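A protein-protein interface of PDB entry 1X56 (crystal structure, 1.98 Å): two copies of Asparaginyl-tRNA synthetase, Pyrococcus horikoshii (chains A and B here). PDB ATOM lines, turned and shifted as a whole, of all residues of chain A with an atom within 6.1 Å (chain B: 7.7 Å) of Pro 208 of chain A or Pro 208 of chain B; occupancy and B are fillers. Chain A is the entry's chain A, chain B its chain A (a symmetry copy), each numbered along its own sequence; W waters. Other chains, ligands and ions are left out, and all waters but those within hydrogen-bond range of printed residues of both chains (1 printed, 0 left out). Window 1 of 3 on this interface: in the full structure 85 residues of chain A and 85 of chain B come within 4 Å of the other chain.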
ATOM      1  N   ILE A 161      14.885  -0.694 -30.633  1.00  0.00           N
ATOM      2  CA  ILE A 161      14.160   0.437 -31.191  1.00  0.00           C
ATOM      3  C   ILE A 161      15.038   1.687 -31.224  1.00  0.00           C
ATOM      4  O   ILE A 161      15.023   2.418 -32.211  1.00  0.00           O
ATOM      5  CB  ILE A 161      12.819   0.695 -30.400  1.00  0.00           C
ATOM      6  CG1 ILE A 161      11.932  -0.587 -30.296  1.00  0.00           C
ATOM      7  CG2 ILE A 161      12.050   1.886 -30.982  1.00  0.00           C
ATOM      8  CD1 ILE A 161      11.662  -1.331 -31.592  1.00  0.00           C
ATOM      9  N   SER A 186      14.160   3.656 -34.559  1.00  0.00           N
ATOM     10  CA  SER A 186      14.294   2.719 -35.670  1.00  0.00           C
ATOM     11  C   SER A 186      13.171   2.806 -36.715  1.00  0.00           C
ATOM     12  O   SER A 186      11.987   2.979 -36.397  1.00  0.00           O
ATOM     13  CB  SER A 186      14.346   1.307 -35.109  1.00  0.00           C
ATOM     14  OG  SER A 186      14.641   0.407 -36.141  1.00  0.00           O
ATOM     15  N   LEU A 206       8.531  -8.503 -34.660  1.00  0.00           N
ATOM     16  CA  LEU A 206       7.390  -7.640 -34.842  1.00  0.00           C
ATOM     17  C   LEU A 206       7.592  -6.468 -33.902  1.00  0.00           C
ATOM     18  O   LEU A 206       7.519  -6.649 -32.682  1.00  0.00           O
ATOM     19  CB  LEU A 206       6.077  -8.395 -34.552  1.00  0.00           C
ATOM     20  CG  LEU A 206       4.813  -7.526 -34.609  1.00  0.00           C
ATOM     21  CD1 LEU A 206       4.532  -6.990 -36.034  1.00  0.00           C
ATOM     22  CD2 LEU A 206       3.605  -8.336 -34.092  1.00  0.00           C
ATOM     23  N   THR A 207       7.870  -5.284 -34.479  1.00  0.00           N
ATOM     24  CA  THR A 207       8.281  -4.099 -33.694  1.00  0.00           C
ATOM     25  C   THR A 207       7.565  -2.908 -34.268  1.00  0.00           C
ATOM     26  O   THR A 207       7.152  -2.943 -35.456  1.00  0.00           O
ATOM     27  CB  THR A 207       9.830  -3.832 -33.743  1.00  0.00           C
ATOM     28  OG1 THR A 207      10.240  -3.727 -35.114  1.00  0.00           O
ATOM     29  CG2 THR A 207      10.660  -5.090 -33.131  1.00  0.00           C
ATOM     30  N   PRO A 208       7.396  -1.862 -33.451  1.00  0.00           N
ATOM     31  CA  PRO A 208       6.957  -0.577 -33.968  1.00  0.00           C
ATOM     32  C   PRO A 208       8.144   0.091 -34.689  1.00  0.00           C
ATOM     33  O   PRO A 208       9.288   0.016 -34.200  1.00  0.00           O
ATOM     34  CB  PRO A 208       6.526   0.184 -32.722  1.00  0.00           C
ATOM     35  CG  PRO A 208       7.426  -0.415 -31.579  1.00  0.00           C
ATOM     36  CD  PRO A 208       7.580  -1.857 -31.981  1.00  0.00           C
ATOM     37  N   SER A 209       7.887   0.660 -35.872  1.00  0.00           N
ATOM     38  CA  SER A 209       8.883   1.410 -36.649  1.00  0.00           C
ATOM     39  C   SER A 209       8.301   2.764 -36.891  1.00  0.00           C
ATOM     40  O   SER A 209       7.080   2.951 -36.805  1.00  0.00           O
ATOM     41  CB  SER A 209       9.209   0.741 -37.991  1.00  0.00           C
ATOM     42  OG  SER A 209       9.750  -0.583 -37.786  1.00  0.00           O
ATOM     43  N   PHE A 210       9.167   3.723 -37.193  1.00  0.00           N
ATOM     44  CA  PHE A 210       8.809   5.153 -37.114  1.00  0.00           C
ATOM     45  C   PHE A 210       9.225   5.842 -38.394  1.00  0.00           C
ATOM     46  O   PHE A 210      10.252   5.482 -38.961  1.00  0.00           O
ATOM     47  CB  PHE A 210       9.458   5.803 -35.874  1.00  0.00           C
ATOM     48  CG  PHE A 210       9.012   5.171 -34.573  1.00  0.00           C
ATOM     49  CD1 PHE A 210       7.862   5.642 -33.911  1.00  0.00           C
ATOM     50  CD2 PHE A 210       9.682   4.061 -34.065  1.00  0.00           C
ATOM     51  CE1 PHE A 210       7.413   5.010 -32.710  1.00  0.00           C
ATOM     52  CE2 PHE A 210       9.272   3.415 -32.882  1.00  0.00           C
ATOM     53  CZ  PHE A 210       8.133   3.895 -32.188  1.00  0.00           C
ATOM     54  N   GLU A 223       3.973   6.151 -36.991  1.00  0.00           N
ATOM     55  CA  GLU A 223       4.226   4.978 -36.147  1.00  0.00           C
ATOM     56  C   GLU A 223       3.412   3.784 -36.648  1.00  0.00           C
ATOM     57  O   GLU A 223       2.194   3.870 -36.808  1.00  0.00           O
ATOM     58  CB  GLU A 223       3.920   5.281 -34.666  1.00  0.00           C
ATOM     59  CG  GLU A 223       4.099   4.092 -33.723  1.00  0.00           C
ATOM     60  CD  GLU A 223       3.615   4.425 -32.336  1.00  0.00           C
ATOM     61  OE1 GLU A 223       4.164   5.368 -31.755  1.00  0.00           O
ATOM     62  OE2 GLU A 223       2.661   3.783 -31.870  1.00  0.00           O
ATOM     63  N   PHE A 224       4.097   2.669 -36.899  1.00  0.00           N
ATOM     64  CA  PHE A 224       3.404   1.481 -37.459  1.00  0.00           C
ATOM     65  C   PHE A 224       4.072   0.172 -37.024  1.00  0.00           C
ATOM     66  O   PHE A 224       5.214   0.169 -36.578  1.00  0.00           O
ATOM     67  CB  PHE A 224       3.289   1.563 -39.014  1.00  0.00           C
ATOM     68  CG  PHE A 224       4.593   1.384 -39.744  1.00  0.00           C
ATOM     69  CD1 PHE A 224       4.953   0.137 -40.257  1.00  0.00           C
ATOM     70  CD2 PHE A 224       5.486   2.471 -39.896  1.00  0.00           C
ATOM     71  CE1 PHE A 224       6.195  -0.053 -40.921  1.00  0.00           C
ATOM     72  CE2 PHE A 224       6.723   2.304 -40.535  1.00  0.00           C
ATOM     73  CZ  PHE A 224       7.063   1.029 -41.063  1.00  0.00           C
ATOM     74  N   TRP A 225       3.367  -0.931 -37.217  1.00  0.00           N
ATOM     75  CA  TRP A 225       3.864  -2.243 -36.824  1.00  0.00           C
ATOM     76  C   TRP A 225       4.474  -2.981 -38.005  1.00  0.00           C
ATOM     77  O   TRP A 225       3.886  -3.041 -39.069  1.00  0.00           O
ATOM     78  CB  TRP A 225       2.781  -3.029 -36.078  1.00  0.00           C
ATOM     79  CG  TRP A 225       2.650  -2.461 -34.667  1.00  0.00           C
ATOM     80  CD1 TRP A 225       1.933  -1.342 -34.255  1.00  0.00           C
ATOM     81  CD2 TRP A 225       3.344  -2.935 -33.513  1.00  0.00           C
ATOM     82  NE1 TRP A 225       2.131  -1.128 -32.910  1.00  0.00           N
ATOM     83  CE2 TRP A 225       2.965  -2.106 -32.417  1.00  0.00           C
ATOM     84  CE3 TRP A 225       4.230  -4.021 -33.276  1.00  0.00           C
ATOM     85  CZ2 TRP A 225       3.443  -2.321 -31.108  1.00  0.00           C
ATOM     86  CZ3 TRP A 225       4.690  -4.231 -31.976  1.00  0.00           C
ATOM     87  CH2 TRP A 225       4.308  -3.375 -30.917  1.00  0.00           C
ATOM     88  N   HIS A 226       5.674  -3.503 -37.779  1.00  0.00           N
ATOM     89  CA  HIS A 226       6.562  -3.921 -38.828  1.00  0.00           C
ATOM     90  C   HIS A 226       6.899  -5.381 -38.551  1.00  0.00           C
ATOM     91  O   HIS A 226       7.591  -5.688 -37.551  1.00  0.00           O
ATOM     92  CB  HIS A 226       7.835  -3.051 -38.751  1.00  0.00           C
ATOM     93  CG  HIS A 226       8.496  -2.808 -40.075  1.00  0.00           C
ATOM     94  ND1 HIS A 226       9.520  -1.896 -40.234  1.00  0.00           N
ATOM     95  CD2 HIS A 226       8.225  -3.286 -41.316  1.00  0.00           C
ATOM     96  CE1 HIS A 226       9.894  -1.869 -41.506  1.00  0.00           C
ATOM     97  NE2 HIS A 226       9.111  -2.690 -42.190  1.00  0.00           N
ATOM     98  N   PRO B 159      -0.818  -1.006 -28.900  1.00  0.00           N
ATOM     99  CA  PRO B 159      -0.991   0.331 -28.347  1.00  0.00           C
ATOM    100  C   PRO B 159       0.140   1.221 -28.805  1.00  0.00           C
ATOM    101  O   PRO B 159       1.102   0.704 -29.364  1.00  0.00           O
ATOM    102  CB  PRO B 159      -0.901   0.117 -26.808  1.00  0.00           C
ATOM    103  CG  PRO B 159      -0.802  -1.361 -26.631  1.00  0.00           C
ATOM    104  CD  PRO B 159      -0.275  -1.936 -27.893  1.00  0.00           C
ATOM    105  N   PRO B 160      -0.018   2.545 -28.618  1.00  0.00           N
ATOM    106  CA  PRO B 160       0.966   3.542 -29.075  1.00  0.00           C
ATOM    107  C   PRO B 160       2.256   3.575 -28.266  1.00  0.00           C
ATOM    108  O   PRO B 160       2.253   3.339 -27.057  1.00  0.00           O
ATOM    109  CB  PRO B 160       0.208   4.880 -28.947  1.00  0.00           C
ATOM    110  CG  PRO B 160      -0.789   4.621 -27.767  1.00  0.00           C
ATOM    111  CD  PRO B 160      -1.219   3.169 -28.002  1.00  0.00           C
ATOM    112  N   ILE B 161       3.351   3.870 -28.962  1.00  0.00           N
ATOM    113  CA  ILE B 161       4.633   4.117 -28.321  1.00  0.00           C
ATOM    114  C   ILE B 161       4.866   5.614 -28.122  1.00  0.00           C
ATOM    115  O   ILE B 161       5.342   6.023 -27.066  1.00  0.00           O
ATOM    116  CB  ILE B 161       5.810   3.453 -29.137  1.00  0.00           C
ATOM    117  CG1 ILE B 161       5.564   1.935 -29.410  1.00  0.00           C
ATOM    118  CG2 ILE B 161       7.164   3.710 -28.467  1.00  0.00           C
ATOM    119  CD1 ILE B 161       5.188   1.083 -28.210  1.00  0.00           C
ATOM    120  N   LEU B 162       4.554   6.421 -29.145  1.00  0.00           N
ATOM    121  CA  LEU B 162       4.640   7.880 -29.019  1.00  0.00           C
ATOM    122  C   LEU B 162       3.431   8.405 -28.230  1.00  0.00           C
ATOM    123  O   LEU B 162       2.272   8.095 -28.569  1.00  0.00           O
ATOM    124  CB  LEU B 162       4.752   8.542 -30.373  1.00  0.00           C
ATOM    125  CG  LEU B 162       6.105   8.322 -31.075  1.00  0.00           C
ATOM    126  CD1 LEU B 162       5.995   8.865 -32.477  1.00  0.00           C
ATOM    127  CD2 LEU B 162       7.300   8.956 -30.317  1.00  0.00           C
ATOM    128  N   LEU B 185       8.473   8.967 -25.353  1.00  0.00           N
ATOM    129  CA  LEU B 185       8.466   7.523 -25.508  1.00  0.00           C
ATOM    130  C   LEU B 185       7.738   6.858 -24.325  1.00  0.00           C
ATOM    131  O   LEU B 185       8.082   7.068 -23.154  1.00  0.00           O
ATOM    132  CB  LEU B 185       9.905   6.990 -25.657  1.00  0.00           C
ATOM    133  CG  LEU B 185      10.640   7.484 -26.898  1.00  0.00           C
ATOM    134  CD1 LEU B 185      12.005   6.872 -26.926  1.00  0.00           C
ATOM    135  CD2 LEU B 185       9.881   7.101 -28.183  1.00  0.00           C
ATOM    136  N   SER B 186       6.723   6.065 -24.641  1.00  0.00           N
ATOM    137  CA  SER B 186       5.931   5.375 -23.628  1.00  0.00           C
ATOM    138  C   SER B 186       6.755   4.550 -22.628  1.00  0.00           C
ATOM    139  O   SER B 186       7.741   3.886 -22.976  1.00  0.00           O
ATOM    140  CB  SER B 186       4.938   4.461 -24.330  1.00  0.00           C
ATOM    141  OG  SER B 186       4.059   3.917 -23.385  1.00  0.00           O
ATOM    142  N   GLN B 187       6.342   4.595 -21.377  1.00  0.00           N
ATOM    143  CA  GLN B 187       6.944   3.750 -20.374  1.00  0.00           C
ATOM    144  C   GLN B 187       6.042   2.535 -20.056  1.00  0.00           C
ATOM    145  O   GLN B 187       6.432   1.622 -19.338  1.00  0.00           O
ATOM    146  CB  GLN B 187       7.330   4.592 -19.138  1.00  0.00           C
ATOM    147  CG  GLN B 187       6.210   5.063 -18.287  1.00  0.00           C
ATOM    148  CD  GLN B 187       6.729   5.936 -17.122  1.00  0.00           C
ATOM    149  OE1 GLN B 187       7.445   6.931 -17.347  1.00  0.00           O
ATOM    150  NE2 GLN B 187       6.419   5.537 -15.902  1.00  0.00           N
ATOM    151  N   SER B 188       4.840   2.522 -20.644  1.00  0.00           N
ATOM    152  CA  SER B 188       3.791   1.551 -20.318  1.00  0.00           C
ATOM    153  C   SER B 188       2.559   1.757 -21.200  1.00  0.00           C
ATOM    154  O   SER B 188       2.139   2.906 -21.399  1.00  0.00           O
ATOM    155  CB  SER B 188       3.351   1.691 -18.879  1.00  0.00           C
ATOM    156  OG  SER B 188       2.211   0.863 -18.659  1.00  0.00           O
ATOM    157  N   ALA B 189       1.987   0.674 -21.728  1.00  0.00           N
ATOM    158  CA  ALA B 189       0.759   0.787 -22.565  1.00  0.00           C
ATOM    159  C   ALA B 189      -0.519   0.858 -21.728  1.00  0.00           C
ATOM    160  O   ALA B 189      -1.602   0.977 -22.280  1.00  0.00           O
ATOM    161  CB  ALA B 189       0.661  -0.388 -23.510  1.00  0.00           C
ATOM    162  N   SER B 205      -0.886  -6.548 -24.440  1.00  0.00           N
ATOM    163  CA  SER B 205       0.071  -6.107 -25.441  1.00  0.00           C
ATOM    164  C   SER B 205       1.479  -6.453 -25.025  1.00  0.00           C
ATOM    165  O   SER B 205       1.779  -6.688 -23.841  1.00  0.00           O
ATOM    166  CB  SER B 205      -0.067  -4.610 -25.741  1.00  0.00           C
ATOM    167  OG  SER B 205       0.115  -3.859 -24.564  1.00  0.00           O
ATOM    168  N   LEU B 206       2.343  -6.521 -26.034  1.00  0.00           N
ATOM    169  CA  LEU B 206       3.755  -6.715 -25.811  1.00  0.00           C
ATOM    170  C   LEU B 206       4.461  -5.641 -26.616  1.00  0.00           C
ATOM    171  O   LEU B 206       4.440  -5.695 -27.850  1.00  0.00           O
ATOM    172  CB  LEU B 206       4.189  -8.133 -26.232  1.00  0.00           C
ATOM    173  CG  LEU B 206       5.699  -8.395 -26.139  1.00  0.00           C
ATOM    174  CD1 LEU B 206       6.213  -8.355 -24.680  1.00  0.00           C
ATOM    175  CD2 LEU B 206       6.029  -9.757 -26.787  1.00  0.00           C
ATOM    176  N   THR B 207       5.058  -4.664 -25.909  1.00  0.00           N
ATOM    177  CA  THR B 207       5.616  -3.452 -26.548  1.00  0.00           C
ATOM    178  C   THR B 207       6.932  -3.158 -25.885  1.00  0.00           C
ATOM    179  O   THR B 207       7.156  -3.592 -24.725  1.00  0.00           O
ATOM    180  CB  THR B 207       4.684  -2.194 -26.407  1.00  0.00           C
ATOM    181  OG1 THR B 207       4.405  -1.976 -25.017  1.00  0.00           O
ATOM    182  CG2 THR B 207       3.241  -2.452 -27.111  1.00  0.00           C
ATOM    183  N   PRO B 208       7.814  -2.445 -26.596  1.00  0.00           N
ATOM    184  CA  PRO B 208       8.999  -1.886 -25.967  1.00  0.00           C
ATOM    185  C   PRO B 208       8.576  -0.661 -25.132  1.00  0.00           C
ATOM    186  O   PRO B 208       7.722   0.129 -25.578  1.00  0.00           O
ATOM    187  CB  PRO B 208       9.888  -1.512 -27.145  1.00  0.00           C
ATOM    188  CG  PRO B 208       8.873  -1.198 -28.305  1.00  0.00           C
ATOM    189  CD  PRO B 208       7.746  -2.161 -28.049  1.00  0.00           C
ATOM    190  N   SER B 209       9.107  -0.555 -23.908  1.00  0.00           N
ATOM    191  CA  SER B 209       8.877   0.589 -23.017  1.00  0.00           C
ATOM    192  C   SER B 209      10.224   1.127 -22.661  1.00  0.00           C
ATOM    193  O   SER B 209      11.236   0.423 -22.778  1.00  0.00           O
ATOM    194  CB  SER B 209       8.122   0.199 -21.739  1.00  0.00           C
ATOM    195  OG  SER B 209       6.824  -0.349 -22.057  1.00  0.00           O
ATOM    196  N   PHE B 210      10.252   2.380 -22.225  1.00  0.00           N
ATOM    197  CA  PHE B 210      11.505   3.160 -22.171  1.00  0.00           C
ATOM    198  C   PHE B 210      11.629   3.808 -20.810  1.00  0.00           C
ATOM    199  O   PHE B 210      10.617   4.205 -20.241  1.00  0.00           O
ATOM    200  CB  PHE B 210      11.540   4.202 -23.309  1.00  0.00           C
ATOM    201  CG  PHE B 210      11.478   3.577 -24.686  1.00  0.00           C
ATOM    202  CD1 PHE B 210      12.659   3.184 -25.343  1.00  0.00           C
ATOM    203  CD2 PHE B 210      10.247   3.302 -25.277  1.00  0.00           C
ATOM    204  CE1 PHE B 210      12.595   2.546 -26.621  1.00  0.00           C
ATOM    205  CE2 PHE B 210      10.144   2.679 -26.537  1.00  0.00           C
ATOM    206  CZ  PHE B 210      11.326   2.304 -27.224  1.00  0.00           C
ATOM    207  N   THR B 222      17.344   0.920 -20.466  1.00  0.00           N
ATOM    208  CA  THR B 222      16.550   2.103 -20.776  1.00  0.00           C
ATOM    209  C   THR B 222      15.503   1.719 -21.809  1.00  0.00           C
ATOM    210  O   THR B 222      14.582   2.497 -22.094  1.00  0.00           O
ATOM    211  CB  THR B 222      17.415   3.276 -21.320  1.00  0.00           C
ATOM    212  OG1 THR B 222      18.131   2.818 -22.462  1.00  0.00           O
ATOM    213  CG2 THR B 222      18.496   3.676 -20.333  1.00  0.00           C
ATOM    214  N   GLU B 223      15.682   0.534 -22.393  1.00  0.00           N
ATOM    215  CA  GLU B 223      14.722  -0.040 -23.342  1.00  0.00           C
ATOM    216  C   GLU B 223      14.459  -1.508 -23.001  1.00  0.00           C
ATOM    217  O   GLU B 223      15.389  -2.307 -22.885  1.00  0.00           O
ATOM    218  CB  GLU B 223      15.215   0.117 -24.795  1.00  0.00           C
ATOM    219  CG  GLU B 223      14.301  -0.509 -25.848  1.00  0.00           C
ATOM    220  CD  GLU B 223      14.938  -0.464 -27.212  1.00  0.00           C
ATOM    221  OE1 GLU B 223      15.221   0.650 -27.669  1.00  0.00           O
ATOM    222  OE2 GLU B 223      15.199  -1.535 -27.781  1.00  0.00           O
ATOM    223  N   PHE B 224      13.184  -1.855 -22.839  1.00  0.00           N
ATOM    224  CA  PHE B 224      12.836  -3.240 -22.434  1.00  0.00           C
ATOM    225  C   PHE B 224      11.466  -3.667 -22.973  1.00  0.00           C
ATOM    226  O   PHE B 224      10.661  -2.831 -23.370  1.00  0.00           O
ATOM    227  CB  PHE B 224      12.910  -3.422 -20.885  1.00  0.00           C
ATOM    228  CG  PHE B 224      11.817  -2.721 -20.124  1.00  0.00           C
ATOM    229  CD1 PHE B 224      10.672  -3.416 -19.728  1.00  0.00           C
ATOM    230  CD2 PHE B 224      11.921  -1.344 -19.823  1.00  0.00           C
ATOM    231  CE1 PHE B 224       9.619  -2.759 -19.035  1.00  0.00           C
ATOM    232  CE2 PHE B 224      10.889  -0.672 -19.153  1.00  0.00           C
ATOM    233  CZ  PHE B 224       9.739  -1.400 -18.746  1.00  0.00           C
ATOM    234  N   TRP B 225      11.201  -4.962 -22.926  1.00  0.00           N
ATOM    235  CA  TRP B 225       9.950  -5.514 -23.431  1.00  0.00           C
ATOM    236  C   TRP B 225       8.951  -5.739 -22.308  1.00  0.00           C
ATOM    237  O   TRP B 225       9.288  -6.299 -21.281  1.00  0.00           O
ATOM    238  CB  TRP B 225      10.216  -6.747 -24.299  1.00  0.00           C
ATOM    239  CG  TRP B 225      10.763  -6.286 -25.648  1.00  0.00           C
ATOM    240  CD1 TRP B 225      12.072  -5.943 -25.971  1.00  0.00           C
ATOM    241  CD2 TRP B 225       9.983  -6.025 -26.815  1.00  0.00           C
ATOM    242  NE1 TRP B 225      12.134  -5.514 -27.278  1.00  0.00           N
ATOM    243  CE2 TRP B 225      10.877  -5.583 -27.834  1.00  0.00           C
ATOM    244  CE3 TRP B 225       8.603  -6.161 -27.125  1.00  0.00           C
ATOM    245  CZ2 TRP B 225      10.439  -5.269 -29.137  1.00  0.00           C
ATOM    246  CZ3 TRP B 225       8.181  -5.857 -28.420  1.00  0.00           C
ATOM    247  CH2 TRP B 225       9.093  -5.402 -29.400  1.00  0.00           C
ATOM    248  N   HIS B 226       7.734  -5.257 -22.537  1.00  0.00           N
ATOM    249  CA  HIS B 226       6.762  -5.048 -21.500  1.00  0.00           C
ATOM    250  C   HIS B 226       5.519  -5.827 -21.912  1.00  0.00           C
ATOM    251  O   HIS B 226       4.850  -5.464 -22.909  1.00  0.00           O
ATOM    252  CB  HIS B 226       6.452  -3.536 -21.434  1.00  0.00           C
ATOM    253  CG  HIS B 226       6.089  -3.042 -20.065  1.00  0.00           C
ATOM    254  ND1 HIS B 226       5.978  -1.698 -19.770  1.00  0.00           N
ATOM    255  CD2 HIS B 226       5.901  -3.699 -18.892  1.00  0.00           C
ATOM    256  CE1 HIS B 226       5.673  -1.552 -18.487  1.00  0.00           C
ATOM    257  NE2 HIS B 226       5.640  -2.751 -17.926  1.00  0.00           N
ATOM    258  N   LEU B 227       5.212  -6.895 -21.177  1.00  0.00           N
ATOM    259  CA  LEU B 227       4.009  -7.687 -21.455  1.00  0.00           C
ATOM    260  C   LEU B 227       2.963  -7.263 -20.440  1.00  0.00           C
ATOM    261  O   LEU B 227       3.138  -7.512 -19.233  1.00  0.00           O
ATOM    262  CB  LEU B 227       4.283  -9.201 -21.297  1.00  0.00           C
ATOM    263  CG  LEU B 227       3.093 -10.142 -21.464  1.00  0.00           C
ATOM    264  CD1 LEU B 227       2.472 -10.118 -22.883  1.00  0.00           C
ATOM    265  CD2 LEU B 227       3.469 -11.567 -21.082  1.00  0.00           C
ATOM    266  N   GLU B 228       1.850  -6.684 -20.936  1.00  0.00           N
ATOM    267  CA  GLU B 228       0.878  -5.994 -20.096  1.00  0.00           C
ATOM    268  C   GLU B 228      -0.522  -6.524 -20.386  1.00  0.00           C
ATOM    269  O   GLU B 228      -0.856  -6.780 -21.544  1.00  0.00           O
ATOM    270  CB  GLU B 228       0.952  -4.495 -20.389  1.00  0.00           C
ATOM    271  CG  GLU B 228       2.355  -3.960 -20.071  1.00  0.00           C
ATOM    272  CD  GLU B 228       2.516  -2.447 -20.273  1.00  0.00           C
ATOM    273  OE1 GLU B 228       2.359  -1.740 -19.270  1.00  0.00           O
ATOM    274  OE2 GLU B 228       2.814  -1.969 -21.417  1.00  0.00           O
ATOM    275  N   GLU B 407      12.718  -9.209 -19.912  1.00  0.00           N
ATOM    276  CA  GLU B 407      14.136  -9.380 -19.610  1.00  0.00           C
ATOM    277  C   GLU B 407      14.387  -9.705 -18.134  1.00  0.00           C
ATOM    278  O   GLU B 407      15.248 -10.526 -17.836  1.00  0.00           O
ATOM    279  CB  GLU B 407      14.937  -8.140 -19.999  1.00  0.00           C
ATOM    280  CG  GLU B 407      14.992  -7.901 -21.490  1.00  0.00           C
ATOM    281  CD  GLU B 407      13.733  -7.271 -22.071  1.00  0.00           C
ATOM    282  OE1 GLU B 407      12.909  -6.661 -21.366  1.00  0.00           O
ATOM    283  OE2 GLU B 407      13.559  -7.410 -23.292  1.00  0.00           O
HETATM  284  O   HOH W   1       1.637   1.294 -31.876  1.00  0.00           O
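The backbone carbonyl oxygen of Ile 161 of chain A lies within hydrogen-bond range of the backbone NH of Ser 186 of chain A, 2.8 Å away. O of Ile 161 of chain B lies within hydrogen-bond range of N of Ser 186 of chain B (2.8 Å). The backbone NH of Trp 225 of chain B sits at hydrogen-bond distance from the side-chain carboxylate of Glu 407 of chain B. The backbone carbonyl oxygen (O) of Ser 186 of chain A is in hydrogen-bond range of the backbone NH (N) of Phe 210 of chain A, 3.0 Å away. O of Ser 186 of chain B is in hydrogen-bond range of N of Phe 210 of chain B.
Ile 161 of chain A touches Pro 208 of chain B, and with the chains exchanged Pro 208 of chain A touches Ile 161 of chain B. Ile 161 of chain A touches Phe 210 of chain B, and with the chains exchanged Phe 210 of chain A touches Ile 161 of chain B. Ile 161 of chain A touches Glu 223 of chain B, and with the chains exchanged Glu 223 of chain A touches Ile 161 of chain B. Pro 208 of chain A touches its own counterpart, Pro 208 of chain B. Positions printed for both chains: 161, 186, 206, 207, 208, 209, 210, 223, 224, 225 and 226.
Water W1 lies within hydrogen-bond range of the backbone carbonyl oxygen of Pro 159 of chain B (2.6 Å), the indole nitrogen of Trp 225 of chain A (2.7 Å) and the side-chain carboxylate of Glu 223 of chain A (2.7 Å).
The side-chain carboxylate (OE2) of Glu 223 of chain A sits at hydrogen-bond distance from the backbone NH (N) of Ile 161 of chain B, at 3.0 Å. The side-chain carboxylate (OE2) of Glu 223 of chain B sits at hydrogen-bond distance from the backbone NH (N) of Ile 161 of chain A (3.0 Å). The backbone NH (N) of Leu 162 of chain B sits at hydrogen-bond distance from the side-chain carboxylate (OE1) of Glu 223 of chain A, 2.8 Å away.
Of the 23 printed residues of chain B, 8 touch a printed residue of chain A. Printed residues of chain A that touch a printed residue of chain B: Ile 161, Leu 206, Pro 208, Phe 210, Glu 223 and Trp 225. Hydrophobic or aromatic side chains of chain A that line the printed part of chain B: Ile 161, Pro 208, Phe 210 and Trp 225.
Pro 208 of chain A touches just these residues of chain B: Ile 161 (3.7 Å) and Pro 208 (3.7 Å). Of chain A, only Ile 161 (3.7 Å) and Pro 208 (3.7 Å) come within 4 Å of Pro 208 of chain B. Of the printed residues of chain A, Leu 206 of chain B touches Trp 225. Of the printed residues of chain A, Ile 161 of chain B touches Pro 208 (3.7 Å), Phe 210 (3.8 Å) and Glu 223 (3.0 Å). Of the printed residues of chain A, Phe 210 of chain B touches Ile 161.
CG of Pro 208 of chain B touches CG1 of Ile 161 of chain A (3.7 Å). CG2 of Ile 161 of chain A touches CZ of Phe 210 of chain B (3.8 Å). Leu 206 of chain A touches Trp 225 of chain B (O to CH2, 3.8 Å). Ile 161 of chain B touches Pro 208 of chain A. Pro 208 of chain A touches Pro 208 of chain B (CG to CG, 3.7 Å). Ile 161 of chain B touches Phe 210 of chain A. Phe 210 of chain A touches Leu 162 of chain B (CE1 to CG, 3.9 Å). Glu 223 of chain A touches Pro 160 of chain B. Trp 225 of chain A touches Leu 206 of chain B.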
